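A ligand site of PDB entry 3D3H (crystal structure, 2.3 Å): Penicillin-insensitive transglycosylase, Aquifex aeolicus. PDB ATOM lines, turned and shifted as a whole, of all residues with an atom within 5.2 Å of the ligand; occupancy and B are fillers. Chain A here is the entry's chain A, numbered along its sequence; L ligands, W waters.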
ATOM      1  N   GLU A  40      11.496 -23.290  33.378  1.00  0.00           N
ATOM      2  CA  GLU A  40      10.059 -23.096  33.497  1.00  0.00           C
ATOM      3  C   GLU A  40       9.258 -23.963  34.458  1.00  0.00           C
ATOM      4  O   GLU A  40       8.234 -23.512  34.992  1.00  0.00           O
ATOM      5  CB  GLU A  40       9.430 -23.229  32.097  1.00  0.00           C
ATOM      6  CG  GLU A  40       9.875 -22.178  31.120  1.00  0.00           C
ATOM      7  CD  GLU A  40       9.297 -20.814  31.435  1.00  0.00           C
ATOM      8  OE1 GLU A  40       9.908 -19.806  31.023  1.00  0.00           O
ATOM      9  OE2 GLU A  40       8.228 -20.749  32.075  1.00  0.00           O
ATOM     10  N   GLN A  70       8.385 -14.238  40.286  1.00  0.00           N
ATOM     11  CA  GLN A  70       8.463 -15.680  40.079  1.00  0.00           C
ATOM     12  C   GLN A  70       7.084 -16.278  39.837  1.00  0.00           C
ATOM     13  O   GLN A  70       6.210 -16.198  40.693  1.00  0.00           O
ATOM     14  CB  GLN A  70       9.108 -16.351  41.286  1.00  0.00           C
ATOM     15  CG  GLN A  70       9.314 -17.865  41.131  1.00  0.00           C
ATOM     16  CD  GLN A  70      10.316 -18.216  40.051  1.00  0.00           C
ATOM     17  OE1 GLN A  70      10.113 -17.921  38.869  1.00  0.00           O
ATOM     18  NE2 GLN A  70      11.413 -18.856  40.448  1.00  0.00           N
ATOM     19  N   GLY A  71       6.899 -16.872  38.656  1.00  0.00           N
ATOM     20  CA  GLY A  71       5.630 -17.486  38.310  1.00  0.00           C
ATOM     21  C   GLY A  71       5.505 -18.867  38.914  1.00  0.00           C
ATOM     22  O   GLY A  71       6.486 -19.426  39.412  1.00  0.00           O
ATOM     23  N   GLY A  72       4.296 -19.423  38.880  1.00  0.00           N
ATOM     24  CA  GLY A  72       4.088 -20.745  39.453  1.00  0.00           C
ATOM     25  C   GLY A  72       3.391 -21.718  38.521  1.00  0.00           C
ATOM     26  O   GLY A  72       3.012 -22.821  38.928  1.00  0.00           O
ATOM     27  N   SER A  73       3.223 -21.317  37.272  1.00  0.00           N
ATOM     28  CA  SER A  73       2.559 -22.155  36.277  1.00  0.00           C
ATOM     29  C   SER A  73       3.479 -23.242  35.738  1.00  0.00           C
ATOM     30  O   SER A  73       4.676 -23.031  35.560  1.00  0.00           O
ATOM     31  CB  SER A  73       2.034 -21.291  35.125  1.00  0.00           C
ATOM     32  OG  SER A  73       3.043 -20.458  34.595  1.00  0.00           O
ATOM     33  N   GLN A  78       1.072 -23.867  30.480  1.00  0.00           N
ATOM     34  CA  GLN A  78       1.442 -22.967  29.395  1.00  0.00           C
ATOM     35  C   GLN A  78       0.937 -23.557  28.076  1.00  0.00           C
ATOM     36  O   GLN A  78       0.459 -22.841  27.216  1.00  0.00           O
ATOM     37  CB  GLN A  78       2.967 -22.799  29.326  1.00  0.00           C
ATOM     38  CG  GLN A  78       3.578 -22.301  30.616  1.00  0.00           C
ATOM     39  CD  GLN A  78       5.083 -22.097  30.537  1.00  0.00           C
ATOM     40  OE1 GLN A  78       5.768 -22.079  31.560  1.00  0.00           O
ATOM     41  NE2 GLN A  78       5.607 -21.953  29.325  1.00  0.00           N
ATOM     42  N   LYS A  81      -2.703 -22.866  28.036  1.00  0.00           N
ATOM     43  CA  LYS A  81      -2.948 -21.446  27.842  1.00  0.00           C
ATOM     44  C   LYS A  81      -2.877 -21.045  26.366  1.00  0.00           C
ATOM     45  O   LYS A  81      -3.653 -20.208  25.896  1.00  0.00           O
ATOM     46  CB  LYS A  81      -1.937 -20.630  28.655  1.00  0.00           C
ATOM     47  CG  LYS A  81      -2.127 -19.122  28.552  1.00  0.00           C
ATOM     48  CD  LYS A  81      -1.105 -18.344  29.390  1.00  0.00           C
ATOM     49  CE  LYS A  81       0.296 -18.461  28.832  1.00  0.00           C
ATOM     50  NZ  LYS A  81       1.264 -17.553  29.515  1.00  0.00           N
ATOM     51  N   ASN A  82      -1.936 -21.638  25.650  1.00  0.00           N
ATOM     52  CA  ASN A  82      -1.743 -21.325  24.240  1.00  0.00           C
ATOM     53  C   ASN A  82      -2.656 -22.106  23.300  1.00  0.00           C
ATOM     54  O   ASN A  82      -2.525 -22.020  22.086  1.00  0.00           O
ATOM     55  CB  ASN A  82      -0.266 -21.552  23.872  1.00  0.00           C
ATOM     56  CG  ASN A  82       0.682 -20.653  24.656  1.00  0.00           C
ATOM     57  OD1 ASN A  82       1.724 -21.096  25.141  1.00  0.00           O
ATOM     58  ND2 ASN A  82       0.315 -19.384  24.785  1.00  0.00           N
ATOM     59  N   ARG A  89      -6.320 -12.553  30.184  1.00  0.00           N
ATOM     60  CA  ARG A  89      -5.723 -13.061  31.417  1.00  0.00           C
ATOM     61  C   ARG A  89      -6.558 -12.814  32.662  1.00  0.00           C
ATOM     62  O   ARG A  89      -6.089 -12.232  33.637  1.00  0.00           O
ATOM     63  CB  ARG A  89      -4.313 -12.460  31.610  1.00  0.00           C
ATOM     64  CG  ARG A  89      -3.342 -12.756  30.471  1.00  0.00           C
ATOM     65  CD  ARG A  89      -3.364 -14.229  30.088  1.00  0.00           C
ATOM     66  NE  ARG A  89      -3.019 -15.108  31.198  1.00  0.00           N
ATOM     67  CZ  ARG A  89      -3.455 -16.360  31.329  1.00  0.00           C
ATOM     68  NH1 ARG A  89      -3.084 -17.091  32.369  1.00  0.00           N
ATOM     69  NH2 ARG A  89      -4.274 -16.876  30.417  1.00  0.00           N
ATOM     70  N   THR A  90      -7.794 -13.289  32.636  1.00  0.00           N
ATOM     71  CA  THR A  90      -8.687 -13.143  33.779  1.00  0.00           C
ATOM     72  C   THR A  90      -8.556 -14.364  34.692  1.00  0.00           C
ATOM     73  O   THR A  90      -8.066 -15.414  34.266  1.00  0.00           O
ATOM     74  CB  THR A  90     -10.158 -13.006  33.335  1.00  0.00           C
ATOM     75  OG1 THR A  90     -10.546 -14.152  32.569  1.00  0.00           O
ATOM     76  CG2 THR A  90     -10.336 -11.748  32.484  1.00  0.00           C
ATOM     77  N   LEU A  91      -8.967 -14.214  35.946  1.00  0.00           N
ATOM     78  CA  LEU A  91      -8.905 -15.319  36.892  1.00  0.00           C
ATOM     79  C   LEU A  91      -9.795 -16.425  36.355  1.00  0.00           C
ATOM     80  O   LEU A  91      -9.522 -17.609  36.530  1.00  0.00           O
ATOM     81  CB  LEU A  91      -9.392 -14.863  38.265  1.00  0.00           C
ATOM     82  CG  LEU A  91      -9.109 -15.757  39.484  1.00  0.00           C
ATOM     83  CD1 LEU A  91      -9.666 -15.083  40.719  1.00  0.00           C
ATOM     84  CD2 LEU A  91      -9.743 -17.129  39.326  1.00  0.00           C
ATOM     85  N   LYS A  94      -7.802 -18.544  33.947  1.00  0.00           N
ATOM     86  CA  LYS A  94      -6.621 -19.169  34.516  1.00  0.00           C
ATOM     87  C   LYS A  94      -7.100 -20.530  35.046  1.00  0.00           C
ATOM     88  O   LYS A  94      -6.389 -21.546  34.927  1.00  0.00           O
ATOM     89  CB  LYS A  94      -6.035 -18.337  35.653  1.00  0.00           C
ATOM     90  CG  LYS A  94      -4.791 -18.976  36.278  1.00  0.00           C
ATOM     91  CD  LYS A  94      -3.737 -19.272  35.210  1.00  0.00           C
ATOM     92  CE  LYS A  94      -2.605 -20.162  35.728  1.00  0.00           C
ATOM     93  NZ  LYS A  94      -1.713 -19.499  36.727  1.00  0.00           N
ATOM     94  N   TYR A 117       4.570 -29.114  23.580  1.00  0.00           N
ATOM     95  CA  TYR A 117       4.972 -27.827  24.124  1.00  0.00           C
ATOM     96  C   TYR A 117       6.175 -27.232  23.384  1.00  0.00           C
ATOM     97  O   TYR A 117       6.140 -26.074  22.971  1.00  0.00           O
ATOM     98  CB  TYR A 117       5.313 -27.996  25.606  1.00  0.00           C
ATOM     99  CG  TYR A 117       5.923 -26.772  26.252  1.00  0.00           C
ATOM    100  CD1 TYR A 117       5.155 -25.648  26.534  1.00  0.00           C
ATOM    101  CD2 TYR A 117       7.276 -26.767  26.610  1.00  0.00           C
ATOM    102  CE1 TYR A 117       5.718 -24.520  27.163  1.00  0.00           C
ATOM    103  CE2 TYR A 117       7.848 -25.659  27.232  1.00  0.00           C
ATOM    104  CZ  TYR A 117       7.069 -24.543  27.508  1.00  0.00           C
ATOM    105  OH  TYR A 117       7.638 -23.470  28.175  1.00  0.00           O
ATOM    106  N   ILE A 121       5.585 -23.503  21.388  1.00  0.00           N
ATOM    107  CA  ILE A 121       6.080 -22.312  22.080  1.00  0.00           C
ATOM    108  C   ILE A 121       6.585 -21.166  21.192  1.00  0.00           C
ATOM    109  O   ILE A 121       7.456 -21.353  20.339  1.00  0.00           O
ATOM    110  CB  ILE A 121       7.198 -22.743  23.069  1.00  0.00           C
ATOM    111  CG1 ILE A 121       7.680 -21.557  23.891  1.00  0.00           C
ATOM    112  CG2 ILE A 121       8.359 -23.371  22.315  1.00  0.00           C
ATOM    113  CD1 ILE A 121       6.658 -21.046  24.880  1.00  0.00           C
ATOM    114  N   TYR A 122       6.033 -19.972  21.355  1.00  0.00           N
ATOM    115  CA  TYR A 122       6.506 -18.836  20.574  1.00  0.00           C
ATOM    116  C   TYR A 122       7.834 -18.378  21.171  1.00  0.00           C
ATOM    117  O   TYR A 122       7.923 -18.099  22.367  1.00  0.00           O
ATOM    118  CB  TYR A 122       5.511 -17.672  20.582  1.00  0.00           C
ATOM    119  CG  TYR A 122       5.978 -16.518  19.714  1.00  0.00           C
ATOM    120  CD1 TYR A 122       6.181 -16.697  18.341  1.00  0.00           C
ATOM    121  CD2 TYR A 122       6.290 -15.280  20.268  1.00  0.00           C
ATOM    122  CE1 TYR A 122       6.672 -15.664  17.542  1.00  0.00           C
ATOM    123  CE2 TYR A 122       6.778 -14.242  19.482  1.00  0.00           C
ATOM    124  CZ  TYR A 122       6.976 -14.437  18.121  1.00  0.00           C
ATOM    125  OH  TYR A 122       7.461 -13.422  17.336  1.00  0.00           O
ATOM    126  N   TYR A 128       7.950 -20.257  15.939  1.00  0.00           N
ATOM    127  CA  TYR A 128       7.116 -21.056  16.844  1.00  0.00           C
ATOM    128  C   TYR A 128       7.721 -22.450  16.886  1.00  0.00           C
ATOM    129  O   TYR A 128       7.758 -23.113  15.867  1.00  0.00           O
ATOM    130  CB  TYR A 128       5.679 -21.171  16.329  1.00  0.00           C
ATOM    131  CG  TYR A 128       4.887 -19.892  16.398  1.00  0.00           C
ATOM    132  CD1 TYR A 128       5.038 -18.911  15.434  1.00  0.00           C
ATOM    133  CD2 TYR A 128       4.014 -19.646  17.459  1.00  0.00           C
ATOM    134  CE1 TYR A 128       4.347 -17.722  15.511  1.00  0.00           C
ATOM    135  CE2 TYR A 128       3.315 -18.460  17.552  1.00  0.00           C
ATOM    136  CZ  TYR A 128       3.493 -17.488  16.573  1.00  0.00           C
ATOM    137  OH  TYR A 128       2.827 -16.285  16.672  1.00  0.00           O
ATOM    138  N   PRO A 157      10.780 -17.848  26.412  1.00  0.00           N
ATOM    139  CA  PRO A 157       9.371 -17.954  26.811  1.00  0.00           C
ATOM    140  C   PRO A 157       8.835 -16.897  27.781  1.00  0.00           C
ATOM    141  O   PRO A 157       7.699 -16.464  27.659  1.00  0.00           O
ATOM    142  CB  PRO A 157       9.284 -19.370  27.381  1.00  0.00           C
ATOM    143  CG  PRO A 157      10.279 -20.124  26.523  1.00  0.00           C
ATOM    144  CD  PRO A 157      11.455 -19.159  26.481  1.00  0.00           C
ATOM    145  N   LYS A 158       9.655 -16.490  28.752  1.00  0.00           N
ATOM    146  CA  LYS A 158       9.240 -15.476  29.723  1.00  0.00           C
ATOM    147  C   LYS A 158       8.744 -14.211  29.027  1.00  0.00           C
ATOM    148  O   LYS A 158       7.772 -13.598  29.467  1.00  0.00           O
ATOM    149  CB  LYS A 158      10.426 -15.135  30.634  1.00  0.00           C
ATOM    150  CG  LYS A 158      10.150 -14.031  31.642  1.00  0.00           C
ATOM    151  CD  LYS A 158      11.426 -13.685  32.382  1.00  0.00           C
ATOM    152  CE  LYS A 158      11.183 -12.632  33.470  1.00  0.00           C
ATOM    153  NZ  LYS A 158      10.326 -13.165  34.566  1.00  0.00           N
ATOM    154  N   ALA A 159       9.434 -13.816  27.963  1.00  0.00           N
ATOM    155  CA  ALA A 159       9.081 -12.631  27.186  1.00  0.00           C
ATOM    156  C   ALA A 159      10.034 -12.584  25.992  1.00  0.00           C
ATOM    157  O   ALA A 159      11.105 -11.998  26.067  1.00  0.00           O
ATOM    158  CB  ALA A 159       9.241 -11.379  28.045  1.00  0.00           C
ATOM    159  N   PRO A 160       9.633 -13.194  24.855  1.00  0.00           N
ATOM    160  CA  PRO A 160      10.440 -13.231  23.630  1.00  0.00           C
ATOM    161  C   PRO A 160      10.968 -11.891  23.140  1.00  0.00           C
ATOM    162  O   PRO A 160      12.146 -11.775  22.796  1.00  0.00           O
ATOM    163  CB  PRO A 160       9.503 -13.890  22.621  1.00  0.00           C
ATOM    164  CG  PRO A 160       8.636 -14.765  23.481  1.00  0.00           C
ATOM    165  CD  PRO A 160       8.346 -13.875  24.671  1.00  0.00           C
ATOM    166  N   ALA A 161      10.111 -10.870  23.100  1.00  0.00           N
ATOM    167  CA  ALA A 161      10.532  -9.552  22.630  1.00  0.00           C
ATOM    168  C   ALA A 161      11.410  -8.796  23.620  1.00  0.00           C
ATOM    169  O   ALA A 161      12.190  -7.931  23.235  1.00  0.00           O
ATOM    170  CB  ALA A 161       9.316  -8.709  22.277  1.00  0.00           C
ATOM    171  N   LYS A 162      11.286  -9.128  24.903  1.00  0.00           N
ATOM    172  CA  LYS A 162      12.067  -8.468  25.936  1.00  0.00           C
ATOM    173  C   LYS A 162      13.477  -9.062  26.049  1.00  0.00           C
ATOM    174  O   LYS A 162      14.421  -8.364  26.402  1.00  0.00           O
ATOM    175  CB  LYS A 162      11.337  -8.552  27.270  1.00  0.00           C
ATOM    176  CG  LYS A 162      12.063  -7.934  28.465  1.00  0.00           C
ATOM    177  CD  LYS A 162      11.128  -7.889  29.679  1.00  0.00           C
ATOM    178  CE  LYS A 162      11.893  -7.676  30.980  1.00  0.00           C
ATOM    179  NZ  LYS A 162      12.679  -6.424  30.983  1.00  0.00           N
HETATM  180  O1  LIG L   1      -2.058 -15.508  34.803  1.00  0.00           O
HETATM  181  C1  LIG L   1      -0.625 -15.488  34.691  1.00  0.00           C
HETATM  182  C2  LIG L   1       0.069 -16.651  35.484  1.00  0.00           C
HETATM  183  O2  LIG L   1      -0.420 -17.007  36.593  1.00  0.00           O
HETATM  184  O3  LIG L   1       1.079 -17.194  34.984  1.00  0.00           O
HETATM  185  C3  LIG L   1      -0.270 -15.518  33.193  1.00  0.00           C
HETATM  186  O4  LIG L   1       0.006 -14.213  32.639  1.00  0.00           O
HETATM  187  P1  LIG L   1       0.704 -14.143  31.174  1.00  0.00           P
HETATM  188  O5  LIG L   1      -0.196 -14.938  30.079  1.00  0.00           O
HETATM  189  O6  LIG L   1       0.823 -12.722  30.746  1.00  0.00           O
HETATM  190  O7  LIG L   1       2.071 -14.957  31.327  1.00  0.00           O
HETATM  191  C4  LIG L   1       3.325 -14.296  31.583  1.00  0.00           C
HETATM  192  O8  LIG L   1       3.602 -13.987  33.033  1.00  0.00           O
HETATM  193  C5  LIG L   1       3.638 -15.182  33.940  1.00  0.00           C
HETATM  194  C6  LIG L   1       3.694 -14.702  35.428  1.00  0.00           C
HETATM  195  O9  LIG L   1       3.721 -15.538  36.322  1.00  0.00           O
HETATM  196  N1  LIG L   1       3.698 -13.401  35.683  1.00  0.00           N
HETATM  197  C7  LIG L   1       4.923 -16.055  33.453  1.00  0.00           C
HETATM  198  O10 LIG L   1       4.966 -17.226  34.291  1.00  0.00           O
HETATM  199  C8  LIG L   1       6.285 -15.292  33.626  1.00  0.00           C
HETATM  200  C9  LIG L   1       4.670 -16.437  31.929  1.00  0.00           C
HETATM  201  O11 LIG L   1       5.727 -17.218  31.262  1.00  0.00           O
HETATM  202  C10 LIG L   1       5.418 -18.488  30.784  1.00  0.00           C
HETATM  203  O12 LIG L   1       4.276 -18.977  30.889  1.00  0.00           O
HETATM  204  N2  LIG L   1       6.399 -19.145  30.200  1.00  0.00           N
HETATM  205  C11 LIG L   1       4.419 -15.196  30.978  1.00  0.00           C
HETATM  206  O13 LIG L   1       4.036 -15.738  29.679  1.00  0.00           O
HETATM  207  C12 LIG L   1       4.686 -15.083  28.565  1.00  0.00           C
HETATM  208  C13 LIG L   1       4.224 -15.785  27.261  1.00  0.00           C
HETATM  209  C14 LIG L   1       4.901 -15.095  26.023  1.00  0.00           C
HETATM  210  O14 LIG L   1       4.502 -15.738  24.814  1.00  0.00           O
HETATM  211  N3  LIG L   1       4.620 -17.229  27.284  1.00  0.00           N
HETATM  212  C15 LIG L   1       3.807 -18.267  27.052  1.00  0.00           C
HETATM  213  C16 LIG L   1       4.472 -19.626  27.145  1.00  0.00           C
HETATM  214  O15 LIG L   1       2.598 -18.196  26.783  1.00  0.00           O
HETATM  215  O16 LIG L   1       4.311 -13.656  28.530  1.00  0.00           O
HETATM  216  C17 LIG L   1       4.966 -12.930  27.374  1.00  0.00           C
HETATM  217  C18 LIG L   1       4.594 -11.457  27.375  1.00  0.00           C
HETATM  218  O17 LIG L   1       3.705 -11.018  28.425  1.00  0.00           O
HETATM  219  C19 LIG L   1       4.496 -13.567  26.011  1.00  0.00           C
HETATM  220  O18 LIG L   1       5.130 -12.906  24.838  1.00  0.00           O
HETATM  221  C20 LIG L   1       3.283  -9.668  28.125  1.00  0.00           C
HETATM  222  O19 LIG L   1       3.307  -8.868  29.395  1.00  0.00           O
HETATM  223  C21 LIG L   1       3.036  -7.394  29.151  1.00  0.00           C
HETATM  224  C22 LIG L   1       3.228  -6.564  30.447  1.00  0.00           C
HETATM  225  O20 LIG L   1       3.786  -7.367  31.497  1.00  0.00           O
HETATM  226  C23 LIG L   1       1.554  -7.257  28.543  1.00  0.00           C
HETATM  227  O21 LIG L   1       1.208  -5.889  28.273  1.00  0.00           O
HETATM  228  C24 LIG L   1       1.444  -8.125  27.223  1.00  0.00           C
HETATM  229  O22 LIG L   1       0.116  -8.087  26.675  1.00  0.00           O
HETATM  230  C25 LIG L   1       1.816  -9.616  27.515  1.00  0.00           C
HETATM  231  O23 LIG L   1       1.719 -10.371  26.276  1.00  0.00           O
HETATM  232  C26 LIG L   1       4.076 -12.613  23.861  1.00  0.00           C
HETATM  233  C27 LIG L   1       4.564 -11.455  22.927  1.00  0.00           C
HETATM  234  C28 LIG L   1       3.394 -11.193  21.917  1.00  0.00           C
HETATM  235  O24 LIG L   1       3.812 -10.135  21.079  1.00  0.00           O
HETATM  236  N4  LIG L   1       4.868 -10.220  23.766  1.00  0.00           N
HETATM  237  C29 LIG L   1       6.074  -9.859  24.341  1.00  0.00           C
HETATM  238  C30 LIG L   1       6.011  -8.542  25.118  1.00  0.00           C
HETATM  239  O25 LIG L   1       7.144 -10.483  24.279  1.00  0.00           O
HETATM  240  O26 LIG L   1       3.743 -13.848  23.048  1.00  0.00           O
HETATM  241  C31 LIG L   1       2.668 -13.680  22.016  1.00  0.00           C
HETATM  242  C32 LIG L   1       2.419 -15.018  21.298  1.00  0.00           C
HETATM  243  C33 LIG L   1       3.123 -12.526  21.031  1.00  0.00           C
HETATM  244  O27 LIG L   1       1.999 -12.403  20.032  1.00  0.00           O
HETATM  245  C34 LIG L   1       2.311 -12.079  18.640  1.00  0.00           C
HETATM  246  O28 LIG L   1       2.934 -10.727  18.565  1.00  0.00           O
HETATM  247  C35 LIG L   1       1.079 -11.970  17.595  1.00  0.00           C
HETATM  248  O29 LIG L   1       0.353 -13.215  17.539  1.00  0.00           O
HETATM  249  C36 LIG L   1       1.633 -11.589  16.148  1.00  0.00           C
HETATM  250  O30 LIG L   1       0.571 -11.486  15.184  1.00  0.00           O
HETATM  251  C37 LIG L   1       2.427 -10.224  16.223  1.00  0.00           C
HETATM  252  O31 LIG L   1       1.540  -9.115  16.520  1.00  0.00           O
HETATM  253  C38 LIG L   1       3.545 -10.422  17.298  1.00  0.00           C
HETATM  254  C39 LIG L   1       4.470  -9.244  17.595  1.00  0.00           C
HETATM  255  O32 LIG L   1       5.629  -9.491  18.272  1.00  0.00           O
HETATM  256  N5  LIG L   1       4.097  -8.004  17.194  1.00  0.00           N
HETATM  257  C40 LIG L   1      -3.821 -14.015  35.665  1.00  0.00           C
HETATM  258  C41 LIG L   1      -4.362 -14.102  36.912  1.00  0.00           C
HETATM  259  C42 LIG L   1      -2.750 -16.824  40.713  1.00  0.00           C
HETATM  260  C43 LIG L   1      -3.597 -15.991  40.054  1.00  0.00           C
HETATM  261  C44 LIG L   1      -2.787 -16.881  42.220  1.00  0.00           C
HETATM  262  C45 LIG L   1      -3.636 -15.871  38.547  1.00  0.00           C
HETATM  263  C46 LIG L   1      -1.766 -17.711  39.975  1.00  0.00           C
HETATM  264  C47 LIG L   1      -3.498 -14.393  38.146  1.00  0.00           C
HETATM  265  C48 LIG L   1      -2.337 -14.188  35.376  1.00  0.00           C
HETATM  266  C49 LIG L   1      -5.836 -13.905  37.084  1.00  0.00           C
HETATM  267  O   HOH W   1       0.453 -13.914  27.514  1.00  0.00           O
HETATM  268  O   HOH W   2       0.919 -18.673  32.299  1.00  0.00           O
HETATM  269  O   HOH W   3       6.045 -17.730  24.481  1.00  0.00           O
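An oxygen (O2) of the ligand lies within salt-bridge range of the side-chain amino group (NZ) of Lys 94 (2.8 Å).
An oxygen (O5) of the ligand lies within salt-bridge range of the side-chain amino group (NZ) of Lys 81 (3.0 Å).
O5 of the ligand lies within salt-bridge range of NE of Arg 89.
The side-chain amide nitrogen (ND2) of Asn 82 is in hydrogen-bond range of an oxygen (O15) of the ligand (3.3 Å).
N of Ala 161 is in hydrogen-bond range of O25 of the ligand, at 3.2 Å.
The side-chain carboxylate (OE2) of Glu 40 sits at hydrogen-bond distance from a nitrogen (N2) of the ligand, 3.1 Å away.
A nitrogen (N2) of the ligand lies close to the side-chain amide nitrogen (NE2) of Gln 78 (3.0 Å).
O of Pro 157 lies within hydrogen-bond range of N3 of the ligand (3.2 Å).
NE2 of Gln 78 is in hydrogen-bond range of OH of Tyr 117, 2.8 Å away.
OD1 of Asn 82 lies close to O of Gln 78 (3.0 Å).
OE2 of Glu 40 sits close to OE1 of Gln 78 (2.8 Å).
Residues that only touch the ligand: Leu 91 (3.3 Å), Pro 160 (3.4 Å), Gly 71 (3.4 Å), Ile 121 (3.5 Å), Lys 158 (3.5 Å), Thr 90 (3.7 Å), Ser 73 (3.8 Å) and Ala 159 (3.96 Å).
Hydrophobic or aromatic side chains within 4 Å of the ligand: Leu 91, Ile 121, Pro 160 and Ala 161.
Within 4 Å of the ligand: Glu 40, Gly 71, Ser 73, Gln 78, Lys 81, Asn 82, Arg 89, Thr 90, Leu 91, Lys 94, Ile 121, Pro 157, Lys 158, Ala 159, Pro 160 and Ala 161.
Water W3 bridges an oxygen (O14) of the ligand and the backbone carbonyl oxygen of Tyr 122.
Water W2 bridges the side-chain amino group of Lys 81 and an oxygen (O3) of the ligand.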
